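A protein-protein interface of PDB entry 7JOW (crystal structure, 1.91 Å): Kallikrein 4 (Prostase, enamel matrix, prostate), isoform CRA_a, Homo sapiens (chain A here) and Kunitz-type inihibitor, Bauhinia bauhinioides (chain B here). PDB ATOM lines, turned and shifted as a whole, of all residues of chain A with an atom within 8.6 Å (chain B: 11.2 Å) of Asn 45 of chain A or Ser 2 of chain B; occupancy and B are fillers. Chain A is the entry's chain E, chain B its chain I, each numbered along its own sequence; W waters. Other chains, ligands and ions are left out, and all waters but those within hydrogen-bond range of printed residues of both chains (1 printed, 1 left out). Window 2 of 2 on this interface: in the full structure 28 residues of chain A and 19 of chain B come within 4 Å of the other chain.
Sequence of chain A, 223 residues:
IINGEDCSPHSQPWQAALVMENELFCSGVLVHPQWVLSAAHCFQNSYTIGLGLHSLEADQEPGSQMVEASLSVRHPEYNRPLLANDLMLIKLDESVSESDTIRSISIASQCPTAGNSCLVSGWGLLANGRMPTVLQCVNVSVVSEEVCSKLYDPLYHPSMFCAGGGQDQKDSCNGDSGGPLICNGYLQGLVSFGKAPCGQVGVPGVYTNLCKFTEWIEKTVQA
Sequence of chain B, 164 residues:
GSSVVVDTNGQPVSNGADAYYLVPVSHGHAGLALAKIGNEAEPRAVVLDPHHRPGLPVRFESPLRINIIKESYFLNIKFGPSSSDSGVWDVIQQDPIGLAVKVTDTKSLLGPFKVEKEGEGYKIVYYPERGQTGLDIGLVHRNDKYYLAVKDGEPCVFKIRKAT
The backbone carbonyl oxygen (O) of His 41 of chain A lies within hydrogen-bond range of the side-chain amino group (NZ) of Lys 70 of chain B (3.1 Å). The side-chain hydroxyl (OH) of Tyr 73 of chain B lies within hydrogen-bond range of the backbone carbonyl oxygen (O) of His 41 of chain A (2.7 Å). O of Phe 43 of chain A sits at hydrogen-bond distance from NZ of Lys 70 of chain B (3.1 Å). The side-chain amide nitrogen (NE2) of Gln 44 of chain A is in hydrogen-bond range of the backbone carbonyl oxygen (O) of Ser 2 of chain B, 2.9 Å away. The guanidinium group of Arg 74 of chain A sits close to the backbone NH of Gly 1 of chain B (3.4 Å).
Water W1 bridges the backbone carbonyl oxygen of Ala 40 of chain A and the side-chain amino group of Lys 70 of chain B.
Ser 2 of chain B touches just these residues of chain A: Gln 44 (2.9 Å) and Asn 45 (3.3 Å). Of chain B, only Lys 70 (3.1 Å) comes within 4 Å of Phe 43 of chain A. Of chain B, only Ser 2 (2.9 Å), Val 4 (3.8 Å) and Lys 70 (3.9 Å) come within 4 Å of Gln 44 of chain A. No residue of chain B comes within 4 Å of Ser 46 of chain A. Gly 1 of chain B touches one residue of chain A. No residue of chain A comes within 4 Å of Ser 3 of chain B. Of the printed residues of chain B, His 41 of chain A touches Ile 66 (3.8 Å), Lys 70 (3.1 Å) and Tyr 73 (2.7 Å). Printed residues of chain A within 4 Å of Pro 12 of chain B: Met 20 (3.0 Å). Of the printed residues of chain B, Met 20 of chain A touches Pro 12 and Ile 68. Of the printed residues of chain A, Ile 68 of chain B touches Met 20 and Phe 25. The nearest residue of chain A that does not touch Ser 2 of chain B is Phe 43 of chain A (4.3 Å).
Among the printed residues, merely in contact across the chains: Met 20 of chain A with Pro 12 of chain B (3.0 Å), Met 20 of chain A with Ile 68 of chain B (3.9 Å), Phe 25 of chain A with Ile 66 of chain B (3.4 Å), Phe 25 of chain A with Ile 68 of chain B (3.97 Å), His 41 of chain A with Ile 66 of chain B (3.8 Å), Gln 44 of chain A with Val 4 of chain B (3.8 Å), Gln 44 of chain A with Lys 70 of chain B (3.9 Å) and Asn 45 of chain A with Ser 2 of chain B (3.3 Å).
The backbone NH (N) of Gln 44 of chain A sits at hydrogen-bond distance from the side-chain hydroxyl (OH) of Tyr 47 of chain A (3.0 Å). O of Gly 1 of chain B sits at hydrogen-bond distance from NZ of Lys 70 of chain B, 2.8 Å away.
Printed residues of chain A that touch a printed residue of chain B: Met 20, Phe 25, His 41, Phe 43, Gln 44, Asn 45 and Arg 74. Among the printed residues, 13 pairs touch across the chains. Among the printed residues, no Asp or Glu carboxylate lies within 4 Å of a Lys or Arg side-chain nitrogen of the other chain.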
ATOM      1  N   MET A  20       2.165  29.935  37.033  1.00  0.00           N
ATOM      2  CA  MET A  20       2.703  28.551  36.872  1.00  0.00           C
ATOM      3  C   MET A  20       3.121  28.155  38.267  1.00  0.00           C
ATOM      4  O   MET A  20       3.993  28.864  38.793  1.00  0.00           O
ATOM      5  CB  MET A  20       3.955  28.652  35.971  1.00  0.00           C
ATOM      6  CG  MET A  20       4.151  27.616  34.924  1.00  0.00           C
ATOM      7  SD  MET A  20       5.469  28.220  33.762  1.00  0.00           S
ATOM      8  CE  MET A  20       6.855  28.334  34.867  1.00  0.00           C
ATOM      9  N   PHE A  25       4.106  34.416  35.288  1.00  0.00           N
ATOM     10  CA  PHE A  25       5.162  34.523  34.212  1.00  0.00           C
ATOM     11  C   PHE A  25       4.758  35.474  33.077  1.00  0.00           C
ATOM     12  O   PHE A  25       5.726  35.938  32.380  1.00  0.00           O
ATOM     13  CB  PHE A  25       5.484  33.144  33.629  1.00  0.00           C
ATOM     14  CG  PHE A  25       4.300  32.450  33.003  1.00  0.00           C
ATOM     15  CD1 PHE A  25       3.390  31.756  33.796  1.00  0.00           C
ATOM     16  CD2 PHE A  25       4.126  32.450  31.630  1.00  0.00           C
ATOM     17  CE1 PHE A  25       2.340  31.091  33.195  1.00  0.00           C
ATOM     18  CE2 PHE A  25       3.041  31.834  31.029  1.00  0.00           C
ATOM     19  CZ  PHE A  25       2.150  31.160  31.819  1.00  0.00           C
ATOM     20  N   ALA A  40       1.378  35.485  22.197  1.00  0.00           N
ATOM     21  CA  ALA A  40       1.509  34.112  21.745  1.00  0.00           C
ATOM     22  C   ALA A  40       2.773  33.510  22.337  1.00  0.00           C
ATOM     23  O   ALA A  40       2.780  32.306  22.539  1.00  0.00           O
ATOM     24  CB  ALA A  40       1.557  34.059  20.236  1.00  0.00           C
ATOM     25  N   HIS A  41       3.810  34.285  22.686  1.00  0.00           N
ATOM     26  CA  HIS A  41       5.033  33.605  23.185  1.00  0.00           C
ATOM     27  C   HIS A  41       4.803  33.058  24.600  1.00  0.00           C
ATOM     28  O   HIS A  41       5.716  32.382  25.154  1.00  0.00           O
ATOM     29  CB  HIS A  41       6.192  34.629  23.113  1.00  0.00           C
ATOM     30  CG  HIS A  41       6.175  35.776  24.076  1.00  0.00           C
ATOM     31  ND1 HIS A  41       5.763  37.054  23.690  1.00  0.00           N
ATOM     32  CD2 HIS A  41       6.583  35.896  25.334  1.00  0.00           C
ATOM     33  CE1 HIS A  41       5.955  37.899  24.667  1.00  0.00           C
ATOM     34  NE2 HIS A  41       6.435  37.206  25.752  1.00  0.00           N
ATOM     35  N   CYS A  42       3.735  33.513  25.250  1.00  0.00           N
ATOM     36  CA  CYS A  42       3.338  32.993  26.610  1.00  0.00           C
ATOM     37  C   CYS A  42       2.566  31.667  26.581  1.00  0.00           C
ATOM     38  O   CYS A  42       2.090  31.252  27.634  1.00  0.00           O
ATOM     39  CB  CYS A  42       2.445  34.001  27.353  1.00  0.00           C
ATOM     40  SG  CYS A  42       3.264  35.604  27.602  1.00  0.00           S
ATOM     41  N   PHE A  43       2.320  31.115  25.409  1.00  0.00           N
ATOM     42  CA  PHE A  43       1.587  29.841  25.183  1.00  0.00           C
ATOM     43  C   PHE A  43       2.030  28.780  26.194  1.00  0.00           C
ATOM     44  O   PHE A  43       3.252  28.500  26.347  1.00  0.00           O
ATOM     45  CB  PHE A  43       1.851  29.309  23.784  1.00  0.00           C
ATOM     46  CG  PHE A  43       1.160  27.978  23.568  1.00  0.00           C
ATOM     47  CD1 PHE A  43      -0.190  27.913  23.239  1.00  0.00           C
ATOM     48  CD2 PHE A  43       1.830  26.816  23.847  1.00  0.00           C
ATOM     49  CE1 PHE A  43      -0.830  26.673  23.110  1.00  0.00           C
ATOM     50  CE2 PHE A  43       1.193  25.566  23.719  1.00  0.00           C
ATOM     51  CZ  PHE A  43      -0.124  25.488  23.284  1.00  0.00           C
ATOM     52  N   GLN A  44       1.050  28.120  26.747  1.00  0.00           N
ATOM     53  CA  GLN A  44       1.238  26.916  27.610  1.00  0.00           C
ATOM     54  C   GLN A  44       0.088  25.948  27.248  1.00  0.00           C
ATOM     55  O   GLN A  44      -0.990  26.408  26.805  1.00  0.00           O
ATOM     56  CB  GLN A  44       1.251  27.236  29.111  1.00  0.00           C
ATOM     57  CG  GLN A  44       2.467  27.984  29.656  1.00  0.00           C
ATOM     58  CD  GLN A  44       3.725  27.147  29.626  1.00  0.00           C
ATOM     59  OE1 GLN A  44       3.988  26.349  30.537  1.00  0.00           O
ATOM     60  NE2 GLN A  44       4.420  27.116  28.496  1.00  0.00           N
ATOM     61  N   ASN A  45       0.274  24.646  27.471  1.00  0.00           N
ATOM     62  CA  ASN A  45      -0.787  23.652  27.178  1.00  0.00           C
ATOM     63  C   ASN A  45      -1.944  23.840  28.164  1.00  0.00           C
ATOM     64  O   ASN A  45      -3.028  23.490  27.844  1.00  0.00           O
ATOM     65  CB  ASN A  45      -0.221  22.221  27.236  1.00  0.00           C
ATOM     66  CG  ASN A  45       0.786  22.015  26.151  1.00  0.00           C
ATOM     67  OD1 ASN A  45       0.505  22.210  25.009  1.00  0.00           O
ATOM     68  ND2 ASN A  45       1.975  21.570  26.466  1.00  0.00           N
ATOM     69  N   SER A  46      -1.747  24.354  29.370  1.00  0.00           N
ATOM     70  CA  SER A  46      -2.867  24.728  30.236  1.00  0.00           C
ATOM     71  C   SER A  46      -2.426  25.914  31.083  1.00  0.00           C
ATOM     72  O   SER A  46      -1.183  26.133  31.195  1.00  0.00           O
ATOM     73  CB  SER A  46      -3.384  23.588  31.118  1.00  0.00           C
ATOM     74  OG  SER A  46      -2.286  22.961  31.753  1.00  0.00           O
ATOM     75  N   TYR A  47      -3.394  26.615  31.641  1.00  0.00           N
ATOM     76  CA  TYR A  47      -3.204  27.861  32.401  1.00  0.00           C
ATOM     77  C   TYR A  47      -4.001  27.853  33.711  1.00  0.00           C
ATOM     78  O   TYR A  47      -5.103  27.260  33.774  1.00  0.00           O
ATOM     79  CB  TYR A  47      -3.718  29.039  31.591  1.00  0.00           C
ATOM     80  CG  TYR A  47      -3.121  29.175  30.213  1.00  0.00           C
ATOM     81  CD1 TYR A  47      -3.751  28.593  29.133  1.00  0.00           C
ATOM     82  CD2 TYR A  47      -1.939  29.856  30.002  1.00  0.00           C
ATOM     83  CE1 TYR A  47      -3.228  28.684  27.854  1.00  0.00           C
ATOM     84  CE2 TYR A  47      -1.392  29.974  28.711  1.00  0.00           C
ATOM     85  CZ  TYR A  47      -2.064  29.414  27.626  1.00  0.00           C
ATOM     86  OH  TYR A  47      -1.598  29.470  26.309  1.00  0.00           O
ATOM     87  N   THR A  48      -3.461  28.597  34.684  1.00  0.00           N
ATOM     88  CA  THR A  48      -4.132  29.078  35.892  1.00  0.00           C
ATOM     89  C   THR A  48      -4.123  30.595  35.735  1.00  0.00           C
ATOM     90  O   THR A  48      -2.994  31.190  35.592  1.00  0.00           O
ATOM     91  CB  THR A  48      -3.406  28.596  37.149  1.00  0.00           C
ATOM     92  OG1 THR A  48      -3.329  27.189  37.062  1.00  0.00           O
ATOM     93  CG2 THR A  48      -4.098  28.887  38.463  1.00  0.00           C
ATOM     94  N   ALA A  69      -7.786  27.085  32.408  1.00  0.00           N
ATOM     95  CA  ALA A  69      -8.014  27.116  30.945  1.00  0.00           C
ATOM     96  C   ALA A  69      -7.116  26.098  30.268  1.00  0.00           C
ATOM     97  O   ALA A  69      -5.934  25.967  30.672  1.00  0.00           O
ATOM     98  CB  ALA A  69      -7.747  28.512  30.453  1.00  0.00           C
ATOM     99  N   SER A  70      -7.604  25.416  29.238  1.00  0.00           N
ATOM    100  CA  SER A  70      -6.708  24.530  28.451  1.00  0.00           C
ATOM    101  C   SER A  70      -6.668  24.907  26.971  1.00  0.00           C
ATOM    102  O   SER A  70      -5.573  24.779  26.397  1.00  0.00           O
ATOM    103  CB  SER A  70      -7.050  23.040  28.645  1.00  0.00           C
ATOM    104  OG  SER A  70      -8.459  22.948  28.550  1.00  0.00           O
ATOM    105  N   LEU A  71      -7.711  25.497  26.384  1.00  0.00           N
ATOM    106  CA  LEU A  71      -7.732  25.878  24.954  1.00  0.00           C
ATOM    107  C   LEU A  71      -7.073  27.253  24.791  1.00  0.00           C
ATOM    108  O   LEU A  71      -7.541  28.202  25.433  1.00  0.00           O
ATOM    109  CB  LEU A  71      -9.193  25.921  24.508  1.00  0.00           C
ATOM    110  CG  LEU A  71      -9.468  26.186  23.023  1.00  0.00           C
ATOM    111  CD1 LEU A  71      -9.465  27.622  22.702  1.00  0.00           C
ATOM    112  CD2 LEU A  71      -8.480  25.527  22.075  1.00  0.00           C
ATOM    113  N   SER A  72      -6.069  27.379  23.940  1.00  0.00           N
ATOM    114  CA  SER A  72      -5.543  28.673  23.500  1.00  0.00           C
ATOM    115  C   SER A  72      -5.344  28.654  21.991  1.00  0.00           C
ATOM    116  O   SER A  72      -5.337  27.563  21.406  1.00  0.00           O
ATOM    117  CB  SER A  72      -4.384  29.129  24.328  1.00  0.00           C
ATOM    118  OG  SER A  72      -3.300  28.248  24.459  1.00  0.00           O
ATOM    119  N   ARG A  74      -3.197  30.567  19.036  1.00  0.00           N
ATOM    120  CA  ARG A  74      -2.141  31.490  18.661  1.00  0.00           C
ATOM    121  C   ARG A  74      -2.564  32.048  17.306  1.00  0.00           C
ATOM    122  O   ARG A  74      -3.166  31.331  16.532  1.00  0.00           O
ATOM    123  CB  ARG A  74      -0.808  30.749  18.671  1.00  0.00           C
ATOM    124  CG  ARG A  74      -0.282  30.415  20.069  1.00  0.00           C
ATOM    125  CD  ARG A  74       1.116  29.825  19.942  1.00  0.00           C
ATOM    126  NE  ARG A  74       0.840  28.476  19.618  1.00  0.00           N
ATOM    127  CZ  ARG A  74       1.494  27.370  20.023  1.00  0.00           C
ATOM    128  NH1 ARG A  74       2.677  27.376  20.638  1.00  0.00           N
ATOM    129  NH2 ARG A  74       0.952  26.229  19.710  1.00  0.00           N
ATOM    130  N   MET A  88      -2.436  35.742  21.187  1.00  0.00           N
ATOM    131  CA  MET A  88      -3.178  34.488  21.306  1.00  0.00           C
ATOM    132  C   MET A  88      -4.419  34.700  22.165  1.00  0.00           C
ATOM    133  O   MET A  88      -4.445  35.615  23.004  1.00  0.00           O
ATOM    134  CB  MET A  88      -2.257  33.394  21.850  1.00  0.00           C
ATOM    135  CG  MET A  88      -1.936  33.499  23.255  1.00  0.00           C
ATOM    136  SD  MET A  88      -1.310  31.881  23.953  1.00  0.00           S
ATOM    137  CE  MET A  88      -0.943  32.535  25.541  1.00  0.00           C
ATOM    138  N   ILE A  90      -6.992  32.805  24.843  1.00  0.00           N
ATOM    139  CA  ILE A  90      -7.193  31.707  25.825  1.00  0.00           C
ATOM    140  C   ILE A  90      -8.663  31.623  26.162  1.00  0.00           C
ATOM    141  O   ILE A  90      -9.222  32.602  26.616  1.00  0.00           O
ATOM    142  CB  ILE A  90      -6.361  32.005  27.079  1.00  0.00           C
ATOM    143  CG1 ILE A  90      -4.894  32.202  26.711  1.00  0.00           C
ATOM    144  CG2 ILE A  90      -6.522  30.906  28.130  1.00  0.00           C
ATOM    145  CD1 ILE A  90      -4.113  32.747  27.873  1.00  0.00           C
ATOM    146  N   GLY B   1       5.971  26.939  21.554  1.00  0.00           N
ATOM    147  CA  GLY B   1       6.332  25.623  22.021  1.00  0.00           C
ATOM    148  C   GLY B   1       6.013  25.567  23.493  1.00  0.00           C
ATOM    149  O   GLY B   1       6.272  26.614  24.112  1.00  0.00           O
ATOM    150  N   SER B   2       5.372  24.461  23.953  1.00  0.00           N
ATOM    151  CA  SER B   2       5.131  23.966  25.326  1.00  0.00           C
ATOM    152  C   SER B   2       6.234  24.262  26.378  1.00  0.00           C
ATOM    153  O   SER B   2       5.911  24.810  27.480  1.00  0.00           O
ATOM    154  CB  SER B   2       4.903  22.353  25.257  1.00  0.00           C
ATOM    155  OG  SER B   2       4.577  21.827  23.966  1.00  0.00           O
ATOM    156  N   SER B   3       7.417  23.636  26.199  1.00  0.00           N
ATOM    157  CA  SER B   3       8.279  23.198  27.307  1.00  0.00           C
ATOM    158  C   SER B   3       9.266  24.309  27.717  1.00  0.00           C
ATOM    159  O   SER B   3       9.831  25.082  26.941  1.00  0.00           O
ATOM    160  CB  SER B   3       8.952  21.831  27.110  1.00  0.00           C
ATOM    161  OG  SER B   3       9.488  21.753  25.821  1.00  0.00           O
ATOM    162  N   VAL B   4       9.259  24.429  28.999  1.00  0.00           N
ATOM    163  CA  VAL B   4       9.994  25.416  29.818  1.00  0.00           C
ATOM    164  C   VAL B   4      11.279  24.758  30.195  1.00  0.00           C
ATOM    165  O   VAL B   4      11.205  23.624  30.735  1.00  0.00           O
ATOM    166  CB  VAL B   4       9.119  25.817  31.024  1.00  0.00           C
ATOM    167  CG1 VAL B   4       9.866  26.720  31.953  1.00  0.00           C
ATOM    168  CG2 VAL B   4       7.826  26.491  30.541  1.00  0.00           C
ATOM    169  N   VAL B   5      12.365  25.481  30.043  1.00  0.00           N
ATOM    170  CA  VAL B   5      13.677  25.055  30.563  1.00  0.00           C
ATOM    171  C   VAL B   5      13.673  25.135  32.112  1.00  0.00           C
ATOM    172  O   VAL B   5      13.380  26.240  32.600  1.00  0.00           O
ATOM    173  CB  VAL B   5      14.773  25.908  29.950  1.00  0.00           C
ATOM    174  CG1 VAL B   5      16.113  25.476  30.471  1.00  0.00           C
ATOM    175  CG2 VAL B   5      14.762  25.809  28.435  1.00  0.00           C
ATOM    176  N   VAL B   6      14.119  24.070  32.815  1.00  0.00           N
ATOM    177  CA  VAL B   6      14.165  24.116  34.316  1.00  0.00           C
ATOM    178  C   VAL B   6      15.552  23.854  34.855  1.00  0.00           C
ATOM    179  O   VAL B   6      16.441  23.302  34.132  1.00  0.00           O
ATOM    180  CB  VAL B   6      13.126  23.211  34.948  1.00  0.00           C
ATOM    181  CG1 VAL B   6      11.729  23.634  34.579  1.00  0.00           C
ATOM    182  CG2 VAL B   6      13.254  21.752  34.531  1.00  0.00           C
ATOM    183  N   PRO B  12      11.636  27.001  36.766  1.00  0.00           N
ATOM    184  CA  PRO B  12      11.933  27.618  35.455  1.00  0.00           C
ATOM    185  C   PRO B  12      13.170  28.519  35.490  1.00  0.00           C
ATOM    186  O   PRO B  12      13.449  29.141  36.496  1.00  0.00           O
ATOM    187  CB  PRO B  12      10.695  28.361  35.067  1.00  0.00           C
ATOM    188  CG  PRO B  12       9.650  27.692  35.877  1.00  0.00           C
ATOM    189  CD  PRO B  12      10.278  27.300  37.211  1.00  0.00           C
ATOM    190  N   ILE B  66       8.958  38.139  28.972  1.00  0.00           N
ATOM    191  CA  ILE B  66       8.502  36.983  29.811  1.00  0.00           C
ATOM    192  C   ILE B  66       9.655  36.703  30.754  1.00  0.00           C
ATOM    193  O   ILE B  66      10.802  37.025  30.366  1.00  0.00           O
ATOM    194  CB  ILE B  66       8.088  35.797  28.912  1.00  0.00           C
ATOM    195  CG1 ILE B  66       7.458  34.659  29.707  1.00  0.00           C
ATOM    196  CG2 ILE B  66       9.263  35.308  28.115  1.00  0.00           C
ATOM    197  CD1 ILE B  66       6.888  33.615  28.859  1.00  0.00           C
ATOM    198  N   ILE B  68      10.642  33.680  32.011  1.00  0.00           N
ATOM    199  CA  ILE B  68      11.154  32.295  31.887  1.00  0.00           C
ATOM    200  C   ILE B  68      11.600  32.058  30.465  1.00  0.00           C
ATOM    201  O   ILE B  68      11.253  32.853  29.606  1.00  0.00           O
ATOM    202  CB  ILE B  68      10.037  31.322  32.296  1.00  0.00           C
ATOM    203  CG1 ILE B  68       8.897  31.452  31.319  1.00  0.00           C
ATOM    204  CG2 ILE B  68       9.579  31.553  33.722  1.00  0.00           C
ATOM    205  CD1 ILE B  68       7.745  30.596  31.588  1.00  0.00           C
ATOM    206  N   ILE B  69      12.294  30.965  30.241  1.00  0.00           N
ATOM    207  CA  ILE B  69      12.889  30.522  28.965  1.00  0.00           C
ATOM    208  C   ILE B  69      12.155  29.269  28.558  1.00  0.00           C
ATOM    209  O   ILE B  69      12.145  28.220  29.314  1.00  0.00           O
ATOM    210  CB  ILE B  69      14.389  30.306  29.212  1.00  0.00           C
ATOM    211  CG1 ILE B  69      15.078  31.612  29.588  1.00  0.00           C
ATOM    212  CG2 ILE B  69      15.049  29.694  28.037  1.00  0.00           C
ATOM    213  CD1 ILE B  69      14.912  32.677  28.595  1.00  0.00           C
ATOM    214  N   LYS B  70      11.716  29.287  27.335  1.00  0.00           N
ATOM    215  CA  LYS B  70      11.186  28.072  26.696  1.00  0.00           C
ATOM    216  C   LYS B  70      12.191  27.485  25.701  1.00  0.00           C
ATOM    217  O   LYS B  70      13.095  28.216  25.213  1.00  0.00           O
ATOM    218  CB  LYS B  70       9.895  28.352  25.974  1.00  0.00           C
ATOM    219  CG  LYS B  70       8.775  28.815  26.872  1.00  0.00           C
ATOM    220  CD  LYS B  70       7.529  28.441  26.111  1.00  0.00           C
ATOM    221  CE  LYS B  70       6.388  29.407  26.038  1.00  0.00           C
ATOM    222  NZ  LYS B  70       5.776  29.264  24.722  1.00  0.00           N
ATOM    223  N   GLU B  71      12.082  26.166  25.467  1.00  0.00           N
ATOM    224  CA  GLU B  71      13.058  25.451  24.596  1.00  0.00           C
ATOM    225  C   GLU B  71      12.953  25.980  23.173  1.00  0.00           C
ATOM    226  O   GLU B  71      13.999  25.965  22.465  1.00  0.00           O
ATOM    227  CB  GLU B  71      12.805  23.944  24.577  1.00  0.00           C
ATOM    228  CG  GLU B  71      12.989  23.262  25.869  1.00  0.00           C
ATOM    229  CD  GLU B  71      12.965  21.733  25.790  1.00  0.00           C
ATOM    230  OE1 GLU B  71      13.238  21.122  24.682  1.00  0.00           O
ATOM    231  OE2 GLU B  71      12.630  21.164  26.847  1.00  0.00           O
ATOM    232  N   SER B  72      11.842  26.631  22.773  1.00  0.00           N
ATOM    233  CA  SER B  72      11.611  27.094  21.415  1.00  0.00           C
ATOM    234  C   SER B  72      12.168  28.519  21.219  1.00  0.00           C
ATOM    235  O   SER B  72      12.232  28.936  20.054  1.00  0.00           O
ATOM    236  CB  SER B  72      10.122  27.085  21.128  1.00  0.00           C
ATOM    237  OG  SER B  72       9.468  28.054  21.993  1.00  0.00           O
ATOM    238  N   TYR B  73      12.650  29.205  22.239  1.00  0.00           N
ATOM    239  CA  TYR B  73      13.153  30.566  22.080  1.00  0.00           C
ATOM    240  C   TYR B  73      14.570  30.594  21.516  1.00  0.00           C
ATOM    241  O   TYR B  73      15.439  29.945  22.048  1.00  0.00           O
ATOM    242  CB  TYR B  73      13.172  31.316  23.396  1.00  0.00           C
ATOM    243  CG  TYR B  73      11.854  31.643  24.054  1.00  0.00           C
ATOM    244  CD1 TYR B  73      10.652  31.492  23.396  1.00  0.00           C
ATOM    245  CD2 TYR B  73      11.831  32.095  25.394  1.00  0.00           C
ATOM    246  CE1 TYR B  73       9.464  31.738  24.046  1.00  0.00           C
ATOM    247  CE2 TYR B  73      10.651  32.376  26.028  1.00  0.00           C
ATOM    248  CZ  TYR B  73       9.483  32.225  25.340  1.00  0.00           C
ATOM    249  OH  TYR B  73       8.328  32.558  25.943  1.00  0.00           O
ATOM    250  N   LYS B 114      19.424  27.875  20.952  1.00  0.00           N
ATOM    251  CA  LYS B 114      18.318  27.328  21.733  1.00  0.00           C
ATOM    252  C   LYS B 114      18.848  26.298  22.745  1.00  0.00           C
ATOM    253  O   LYS B 114      20.002  25.745  22.586  1.00  0.00           O
ATOM    254  CB  LYS B 114      17.286  26.652  20.846  1.00  0.00           C
ATOM    255  CG  LYS B 114      16.664  27.573  19.830  1.00  0.00           C
ATOM    256  CD  LYS B 114      15.435  26.960  19.221  1.00  0.00           C
ATOM    257  CE  LYS B 114      14.871  27.912  18.217  1.00  0.00           C
ATOM    258  NZ  LYS B 114      13.556  27.522  17.621  1.00  0.00           N
ATOM    259  N   VAL B 115      18.128  26.197  23.843  1.00  0.00           N
ATOM    260  CA  VAL B 115      18.391  25.176  24.875  1.00  0.00           C
ATOM    261  C   VAL B 115      17.306  24.107  24.724  1.00  0.00           C
ATOM    262  O   VAL B 115      16.151  24.444  24.955  1.00  0.00           O
ATOM    263  CB  VAL B 115      18.404  25.793  26.258  1.00  0.00           C
ATOM    264  CG1 VAL B 115      18.601  24.737  27.306  1.00  0.00           C
ATOM    265  CG2 VAL B 115      19.432  26.858  26.321  1.00  0.00           C
ATOM    266  N   GLU B 116      17.670  22.841  24.442  1.00  0.00           N
ATOM    267  CA  GLU B 116      16.705  21.777  24.082  1.00  0.00           C
ATOM    268  C   GLU B 116      16.969  20.564  24.971  1.00  0.00           C
ATOM    269  O   GLU B 116      18.102  20.253  25.270  1.00  0.00           O
ATOM    270  CB  GLU B 116      16.872  21.366  22.593  1.00  0.00           C
ATOM    271  CG  GLU B 116      16.802  22.627  21.706  1.00  0.00           C
ATOM    272  CD  GLU B 116      16.926  22.350  20.194  1.00  0.00           C
ATOM    273  OE1 GLU B 116      17.118  21.020  19.812  1.00  0.00           O
ATOM    274  OE2 GLU B 116      16.792  23.357  19.430  1.00  0.00           O
ATOM    275  N   LYS B 117      15.908  19.946  25.392  1.00  0.00           N
ATOM    276  CA  LYS B 117      15.940  18.769  26.276  1.00  0.00           C
ATOM    277  C   LYS B 117      16.795  17.674  25.600  1.00  0.00           C
ATOM    278  O   LYS B 117      16.700  17.484  24.390  1.00  0.00           O
ATOM    279  CB  LYS B 117      14.461  18.414  26.486  1.00  0.00           C
ATOM    280  CG  LYS B 117      14.221  17.121  27.199  1.00  0.00           C
ATOM    281  CD  LYS B 117      14.518  17.326  28.599  1.00  0.00           C
ATOM    282  CE  LYS B 117      13.280  17.757  29.358  1.00  0.00           C
ATOM    283  NZ  LYS B 117      12.726  16.600  30.098  1.00  0.00           N
ATOM    284  N   TYR B 122      20.014  19.119  29.275  1.00  0.00           N
ATOM    285  CA  TYR B 122      19.855  20.011  28.094  1.00  0.00           C
ATOM    286  C   TYR B 122      21.126  20.014  27.230  1.00  0.00           C
ATOM    287  O   TYR B 122      22.254  20.045  27.759  1.00  0.00           O
ATOM    288  CB  TYR B 122      19.552  21.413  28.591  1.00  0.00           C
ATOM    289  CG  TYR B 122      18.230  21.497  29.298  1.00  0.00           C
ATOM    290  CD1 TYR B 122      17.083  21.560  28.565  1.00  0.00           C
ATOM    291  CD2 TYR B 122      18.111  21.458  30.686  1.00  0.00           C
ATOM    292  CE1 TYR B 122      15.834  21.511  29.157  1.00  0.00           C
ATOM    293  CE2 TYR B 122      16.857  21.471  31.305  1.00  0.00           C
ATOM    294  CZ  TYR B 122      15.701  21.516  30.548  1.00  0.00           C
ATOM    295  OH  TYR B 122      14.410  21.531  31.089  1.00  0.00           O
HETATM  296  O   HOH W   1       4.564  30.130  21.880  1.00  0.00           O
